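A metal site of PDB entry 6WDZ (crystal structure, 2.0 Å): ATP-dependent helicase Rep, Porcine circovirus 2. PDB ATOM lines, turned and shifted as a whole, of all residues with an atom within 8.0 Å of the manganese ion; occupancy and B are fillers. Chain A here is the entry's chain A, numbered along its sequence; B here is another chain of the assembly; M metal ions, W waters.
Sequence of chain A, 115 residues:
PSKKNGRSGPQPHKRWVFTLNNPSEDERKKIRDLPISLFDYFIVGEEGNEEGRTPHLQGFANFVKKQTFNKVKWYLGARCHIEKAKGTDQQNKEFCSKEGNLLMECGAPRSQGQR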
ATOM      1  N   PHE A  18      14.289   0.260 -12.576  1.00  0.00           N
ATOM      2  CA  PHE A  18      15.343  -0.498 -13.228  1.00  0.00           C
ATOM      3  C   PHE A  18      15.753   0.165 -14.531  1.00  0.00           C
ATOM      4  O   PHE A  18      15.002   0.914 -15.147  1.00  0.00           O
ATOM      5  CB  PHE A  18      14.943  -1.975 -13.462  1.00  0.00           C
ATOM      6  CG  PHE A  18      14.013  -2.197 -14.620  1.00  0.00           C
ATOM      7  CD1 PHE A  18      12.651  -2.008 -14.470  1.00  0.00           C
ATOM      8  CD2 PHE A  18      14.494  -2.616 -15.845  1.00  0.00           C
ATOM      9  CE1 PHE A  18      11.783  -2.253 -15.531  1.00  0.00           C
ATOM     10  CE2 PHE A  18      13.640  -2.842 -16.909  1.00  0.00           C
ATOM     11  CZ  PHE A  18      12.288  -2.650 -16.759  1.00  0.00           C
ATOM     12  N   THR A  19      17.016  -0.046 -14.884  1.00  0.00           N
ATOM     13  CA  THR A  19      17.605   0.295 -16.160  1.00  0.00           C
ATOM     14  C   THR A  19      18.184  -0.996 -16.724  1.00  0.00           C
ATOM     15  O   THR A  19      18.801  -1.766 -15.979  1.00  0.00           O
ATOM     16  CB  THR A  19      18.752   1.315 -16.012  1.00  0.00           C
ATOM     17  OG1 THR A  19      18.298   2.470 -15.285  1.00  0.00           O
ATOM     18  CG2 THR A  19      19.310   1.718 -17.389  1.00  0.00           C
ATOM     19  N   ASN A  21      20.639  -1.852 -19.937  1.00  0.00           N
ATOM     20  CA  ASN A  21      21.361  -1.233 -21.046  1.00  0.00           C
ATOM     21  C   ASN A  21      21.560  -2.229 -22.182  1.00  0.00           C
ATOM     22  O   ASN A  21      21.807  -3.407 -21.959  1.00  0.00           O
ATOM     23  CB  ASN A  21      22.704  -0.678 -20.561  1.00  0.00           C
ATOM     24  CG  ASN A  21      22.583   0.716 -19.940  1.00  0.00           C
ATOM     25  OD1 ASN A  21      22.088   1.626 -20.584  1.00  0.00           O
ATOM     26  ND2 ASN A  21      23.027   0.873 -18.698  1.00  0.00           N
ATOM     27  N   GLY A  45       9.951   2.013 -20.759  1.00  0.00           N
ATOM     28  CA  GLY A  45      10.180   2.832 -21.947  1.00  0.00           C
ATOM     29  C   GLY A  45      11.470   2.457 -22.643  1.00  0.00           C
ATOM     30  O   GLY A  45      12.472   2.146 -21.980  1.00  0.00           O
ATOM     31  N   GLU A  46      11.462   2.512 -23.975  1.00  0.00           N
ATOM     32  CA  GLU A  46      12.694   2.370 -24.759  1.00  0.00           C
ATOM     33  C   GLU A  46      13.334   3.744 -24.872  1.00  0.00           C
ATOM     34  O   GLU A  46      12.708   4.682 -25.363  1.00  0.00           O
ATOM     35  CB  GLU A  46      12.412   1.808 -26.153  1.00  0.00           C
ATOM     36  CG  GLU A  46      11.464   0.620 -26.235  1.00  0.00           C
ATOM     37  CD  GLU A  46      12.187  -0.717 -26.200  1.00  0.00           C
ATOM     38  OE1 GLU A  46      13.408  -0.727 -26.491  1.00  0.00           O
ATOM     39  OE2 GLU A  46      11.543  -1.760 -25.900  1.00  0.00           O
ATOM     40  N   GLU A  47      14.582   3.870 -24.427  1.00  0.00           N
ATOM     41  CA  GLU A  47      15.291   5.134 -24.429  1.00  0.00           C
ATOM     42  C   GLU A  47      16.687   4.941 -25.003  1.00  0.00           C
ATOM     43  O   GLU A  47      17.086   3.826 -25.322  1.00  0.00           O
ATOM     44  CB  GLU A  47      15.363   5.712 -23.016  1.00  0.00           C
ATOM     45  CG  GLU A  47      13.991   6.050 -22.432  1.00  0.00           C
ATOM     46  CD  GLU A  47      14.043   6.709 -21.080  1.00  0.00           C
ATOM     47  OE1 GLU A  47      15.062   6.539 -20.330  1.00  0.00           O
ATOM     48  OE2 GLU A  47      13.044   7.402 -20.759  1.00  0.00           O
ATOM     49  N   GLY A  48      17.439   6.042 -25.094  1.00  0.00           N
ATOM     50  CA  GLY A  48      18.815   5.960 -25.526  1.00  0.00           C
ATOM     51  C   GLY A  48      19.006   5.587 -26.979  1.00  0.00           C
ATOM     52  O   GLY A  48      20.038   5.025 -27.329  1.00  0.00           O
ATOM     53  N   ARG A  53      24.850   7.169 -28.146  1.00  0.00           N
ATOM     54  CA  ARG A  53      24.070   6.969 -26.927  1.00  0.00           C
ATOM     55  C   ARG A  53      23.569   5.541 -26.858  1.00  0.00           C
ATOM     56  O   ARG A  53      23.383   4.897 -27.887  1.00  0.00           O
ATOM     57  CB  ARG A  53      22.982   8.038 -26.869  1.00  0.00           C
ATOM     58  CG  ARG A  53      21.862   7.919 -25.893  1.00  0.00           C
ATOM     59  CD  ARG A  53      21.165   9.270 -25.813  1.00  0.00           C
ATOM     60  NE  ARG A  53      19.759   9.190 -25.388  1.00  0.00           N
ATOM     61  CZ  ARG A  53      19.266   9.049 -24.158  1.00  0.00           C
ATOM     62  NH1 ARG A  53      20.043   8.806 -23.087  1.00  0.00           N
ATOM     63  NH2 ARG A  53      17.946   9.057 -24.039  1.00  0.00           N
ATOM     64  N   THR A  54      23.356   5.069 -25.620  1.00  0.00           N
ATOM     65  CA  THR A  54      23.182   3.648 -25.355  1.00  0.00           C
ATOM     66  C   THR A  54      21.709   3.278 -25.282  1.00  0.00           C
ATOM     67  O   THR A  54      21.001   3.788 -24.400  1.00  0.00           O
ATOM     68  CB  THR A  54      23.899   3.291 -24.047  1.00  0.00           C
ATOM     69  OG1 THR A  54      25.304   3.517 -24.216  1.00  0.00           O
ATOM     70  CG2 THR A  54      23.671   1.862 -23.639  1.00  0.00           C
ATOM     71  N   PRO A  55      21.196   2.436 -26.188  1.00  0.00           N
ATOM     72  CA  PRO A  55      19.799   1.984 -26.080  1.00  0.00           C
ATOM     73  C   PRO A  55      19.570   1.231 -24.784  1.00  0.00           C
ATOM     74  O   PRO A  55      20.366   0.383 -24.392  1.00  0.00           O
ATOM     75  CB  PRO A  55      19.644   1.060 -27.307  1.00  0.00           C
ATOM     76  CG  PRO A  55      20.798   1.406 -28.213  1.00  0.00           C
ATOM     77  CD  PRO A  55      21.909   1.796 -27.307  1.00  0.00           C
ATOM     78  N   HIS A  56      18.481   1.545 -24.094  1.00  0.00           N
ATOM     79  CA  HIS A  56      18.212   0.910 -22.807  1.00  0.00           C
ATOM     80  C   HIS A  56      16.718   0.946 -22.522  1.00  0.00           C
ATOM     81  O   HIS A  56      15.986   1.796 -23.038  1.00  0.00           O
ATOM     82  CB  HIS A  56      18.966   1.555 -21.642  1.00  0.00           C
ATOM     83  CG  HIS A  56      18.700   3.019 -21.477  1.00  0.00           C
ATOM     84  ND1 HIS A  56      19.096   3.951 -22.401  1.00  0.00           N
ATOM     85  CD2 HIS A  56      18.088   3.711 -20.482  1.00  0.00           C
ATOM     86  CE1 HIS A  56      18.761   5.162 -21.985  1.00  0.00           C
ATOM     87  NE2 HIS A  56      18.151   5.041 -20.817  1.00  0.00           N
ATOM     88  N   LEU A  57      16.284   0.023 -21.670  1.00  0.00           N
ATOM     89  CA  LEU A  57      14.946   0.095 -21.068  1.00  0.00           C
ATOM     90  C   LEU A  57      14.988   0.894 -19.771  1.00  0.00           C
ATOM     91  O   LEU A  57      15.904   0.726 -18.960  1.00  0.00           O
ATOM     92  CB  LEU A  57      14.381  -1.300 -20.803  1.00  0.00           C
ATOM     93  CG  LEU A  57      14.263  -2.207 -22.035  1.00  0.00           C
ATOM     94  CD1 LEU A  57      13.497  -3.464 -21.707  1.00  0.00           C
ATOM     95  CD2 LEU A  57      13.603  -1.475 -23.172  1.00  0.00           C
ATOM     96  N   GLN A  58      14.021   1.795 -19.610  1.00  0.00           N
ATOM     97  CA  GLN A  58      13.889   2.641 -18.426  1.00  0.00           C
ATOM     98  C   GLN A  58      12.568   2.268 -17.766  1.00  0.00           C
ATOM     99  O   GLN A  58      11.508   2.535 -18.336  1.00  0.00           O
ATOM    100  CB  GLN A  58      13.883   4.124 -18.795  1.00  0.00           C
ATOM    101  CG  GLN A  58      14.325   5.079 -17.669  1.00  0.00           C
ATOM    102  CD  GLN A  58      15.787   4.918 -17.336  1.00  0.00           C
ATOM    103  OE1 GLN A  58      16.678   5.284 -18.129  1.00  0.00           O
ATOM    104  NE2 GLN A  58      16.050   4.343 -16.160  1.00  0.00           N
ATOM    105  N   GLY A  59      12.630   1.659 -16.584  1.00  0.00           N
ATOM    106  CA  GLY A  59      11.476   0.959 -16.064  1.00  0.00           C
ATOM    107  C   GLY A  59      11.191   1.297 -14.611  1.00  0.00           C
ATOM    108  O   GLY A  59      12.035   1.805 -13.868  1.00  0.00           O
ATOM    109  N   PHE A  95       8.749   9.934 -15.775  1.00  0.00           N
ATOM    110  CA  PHE A  95      10.168   9.795 -16.126  1.00  0.00           C
ATOM    111  C   PHE A  95      10.391   8.693 -17.147  1.00  0.00           C
ATOM    112  O   PHE A  95      11.238   8.843 -18.039  1.00  0.00           O
ATOM    113  CB  PHE A  95      11.010   9.524 -14.872  1.00  0.00           C
ATOM    114  CG  PHE A  95      12.473   9.634 -15.120  1.00  0.00           C
ATOM    115  CD1 PHE A  95      13.056  10.879 -15.279  1.00  0.00           C
ATOM    116  CD2 PHE A  95      13.268   8.508 -15.245  1.00  0.00           C
ATOM    117  CE1 PHE A  95      14.404  11.012 -15.521  1.00  0.00           C
ATOM    118  CE2 PHE A  95      14.624   8.615 -15.477  1.00  0.00           C
ATOM    119  CZ  PHE A  95      15.200   9.877 -15.628  1.00  0.00           C
ATOM    120  N   CYS A  96       9.688   7.571 -17.045  1.00  0.00           N
ATOM    121  CA  CYS A  96       9.927   6.492 -18.002  1.00  0.00           C
ATOM    122  C   CYS A  96       9.141   6.676 -19.298  1.00  0.00           C
ATOM    123  O   CYS A  96       9.318   5.898 -20.222  1.00  0.00           O
ATOM    124  CB  CYS A  96       9.616   5.120 -17.387  1.00  0.00           C
ATOM    125  SG  CYS A  96      10.466   4.788 -15.809  1.00  0.00           S
ATOM    126  N   LYS A  98       9.236   9.709 -20.885  1.00  0.00           N
ATOM    127  CA  LYS A  98       9.742  10.976 -21.394  1.00  0.00           C
ATOM    128  C   LYS A  98      10.308  10.894 -22.810  1.00  0.00           C
ATOM    129  O   LYS A  98      10.471  11.928 -23.453  1.00  0.00           O
ATOM    130  CB  LYS A  98      10.806  11.518 -20.426  1.00  0.00           C
ATOM    131  CG  LYS A  98      12.122  10.734 -20.453  1.00  0.00           C
ATOM    132  CD  LYS A  98      13.067  11.213 -19.353  1.00  0.00           C
ATOM    133  CE  LYS A  98      14.335  10.380 -19.267  1.00  0.00           C
ATOM    134  NZ  LYS A  98      14.029   9.004 -18.787  1.00  0.00           N
ATOM    135  N   GLU A  99      10.631   9.713 -23.321  1.00  0.00           N
ATOM    136  CA  GLU A  99      11.228   9.673 -24.652  1.00  0.00           C
ATOM    137  C   GLU A  99      10.271   9.129 -25.726  1.00  0.00           C
ATOM    138  O   GLU A  99      10.666   9.037 -26.894  1.00  0.00           O
ATOM    139  CB  GLU A  99      12.553   8.879 -24.628  1.00  0.00           C
ATOM    140  CG  GLU A  99      13.637   9.580 -23.753  1.00  0.00           C
ATOM    141  CD  GLU A  99      15.057   9.017 -23.859  1.00  0.00           C
ATOM    142  OE1 GLU A  99      15.356   8.219 -24.765  1.00  0.00           O
ATOM    143  OE2 GLU A  99      15.925   9.398 -23.033  1.00  0.00           O
ATOM    144  P    DT B   7      23.637   9.509 -19.728  1.00  0.00           P
ATOM    145  OP1  DT B   7      23.822   9.238 -21.156  1.00  0.00           O
ATOM    146  OP2  DT B   7      23.215  10.851 -19.313  1.00  0.00           O
ATOM    147  O5'  DT B   7      22.606   8.444 -19.108  1.00  0.00           O
ATOM    148  C5'  DT B   7      21.548   7.949 -19.878  1.00  0.00           C
ATOM    149  C4'  DT B   7      20.943   6.711 -19.218  1.00  0.00           C
ATOM    150  O4'  DT B   7      21.991   5.843 -18.728  1.00  0.00           O
ATOM    151  C3'  DT B   7      20.106   6.997 -18.002  1.00  0.00           C
ATOM    152  O3'  DT B   7      18.791   7.312 -18.415  1.00  0.00           O
ATOM    153  C2'  DT B   7      20.157   5.670 -17.242  1.00  0.00           C
ATOM    154  C1'  DT B   7      21.532   5.105 -17.622  1.00  0.00           C
ATOM    155  N1   DT B   7      22.569   5.185 -16.525  1.00  0.00           N
ATOM    156  C2   DT B   7      23.517   4.194 -16.418  1.00  0.00           C
ATOM    157  O2   DT B   7      23.569   3.230 -17.156  1.00  0.00           O
ATOM    158  N3   DT B   7      24.436   4.373 -15.424  1.00  0.00           N
ATOM    159  C4   DT B   7      24.493   5.403 -14.517  1.00  0.00           C
ATOM    160  O4   DT B   7      25.373   5.455 -13.657  1.00  0.00           O
ATOM    161  C5   DT B   7      23.494   6.436 -14.679  1.00  0.00           C
ATOM    162  C7   DT B   7      23.450   7.628 -13.725  1.00  0.00           C
ATOM    163  C6   DT B   7      22.579   6.274 -15.655  1.00  0.00           C
ATOM    164  P    DA B   8      17.831   8.166 -17.447  1.00  0.00           P
ATOM    165  OP1  DA B   8      16.528   8.063 -18.154  1.00  0.00           O
ATOM    166  OP2  DA B   8      18.509   9.464 -17.156  1.00  0.00           O
ATOM    167  O5'  DA B   8      17.729   7.309 -16.129  1.00  0.00           O
ATOM    168  C5'  DA B   8      18.179   7.819 -14.856  1.00  0.00           C
ATOM    169  C4'  DA B   8      17.979   6.736 -13.803  1.00  0.00           C
ATOM    170  O4'  DA B   8      18.925   5.665 -14.020  1.00  0.00           O
ATOM    171  C3'  DA B   8      18.243   7.148 -12.356  1.00  0.00           C
ATOM    172  O3'  DA B   8      17.157   7.848 -11.829  1.00  0.00           O
ATOM    173  C2'  DA B   8      18.360   5.782 -11.706  1.00  0.00           C
ATOM    174  C1'  DA B   8      19.057   4.963 -12.808  1.00  0.00           C
ATOM    175  N9   DA B   8      20.441   4.658 -12.483  1.00  0.00           N
ATOM    176  C8   DA B   8      21.199   5.214 -11.470  1.00  0.00           C
ATOM    177  N7   DA B   8      22.387   4.675 -11.354  1.00  0.00           N
ATOM    178  C5   DA B   8      22.402   3.671 -12.329  1.00  0.00           C
ATOM    179  C6   DA B   8      23.369   2.735 -12.684  1.00  0.00           C
ATOM    180  N6   DA B   8      24.553   2.657 -12.088  1.00  0.00           N
ATOM    181  N1   DA B   8      23.081   1.855 -13.696  1.00  0.00           N
ATOM    182  C2   DA B   8      21.890   1.950 -14.283  1.00  0.00           C
ATOM    183  N3   DA B   8      20.879   2.793 -14.014  1.00  0.00           N
ATOM    184  C4   DA B   8      21.216   3.623 -13.006  1.00  0.00           C
HETATM  185 MN    MN M   1      16.959   6.597 -19.687  1.00  0.00          MN
HETATM  186  O   HOH W   1      17.640   8.148 -21.078  1.00  0.00           O
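OE2 of Glu 47 is in salt-bridge range of NZ of Lys 98. The side-chain amide nitrogen (NE2) of Gln 58 lies within hydrogen-bond range of the side-chain hydroxyl (OG1) of Thr 19, 3.1 Å away. The backbone NH (N) of Gln 58 is in hydrogen-bond range of the backbone carbonyl oxygen (O) of Gly 45, 2.9 Å away. SG of Cys 96 sits close to O of Gln 58 (3.5 Å). OP1 of DA 8 of chain B lies close to the side-chain amino group (NZ) of Lys 98, at 2.7 Å. N3 of DA 8 of chain B sits at hydrogen-bond distance from OG1 of Thr 19. A ring nitrogen (ND1) of His 56 lies within hydrogen-bond range of the backbone carbonyl oxygen (O) of Thr 54 (2.8 Å). O2 of DT 7 of chain B is in hydrogen-bond range of the side-chain amide nitrogen (ND2) of Asn 21 (2.9 Å).
NZ of Lys 98 touches the manganese ion (3.9 Å). The nearest printed residue that does not touch the manganese ion is Glu 99 (4.5 Å).
The manganese ion is bound by OE1 of Glu 47 (2.0 Å), OE1 of Gln 58 (2.1 Å), OP1 of DA 8 of chain B (2.2 Å), water W1 (2.2 Å), NE2 of His 56 (2.3 Å) and O3' of DT 7 of chain B (2.3 Å). The manganese ion has six donor atoms within binding distance.
Water W1 bridges OE2 of Glu 99 (2.9 Å) and NH2 of Arg 53 (3.1 Å).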
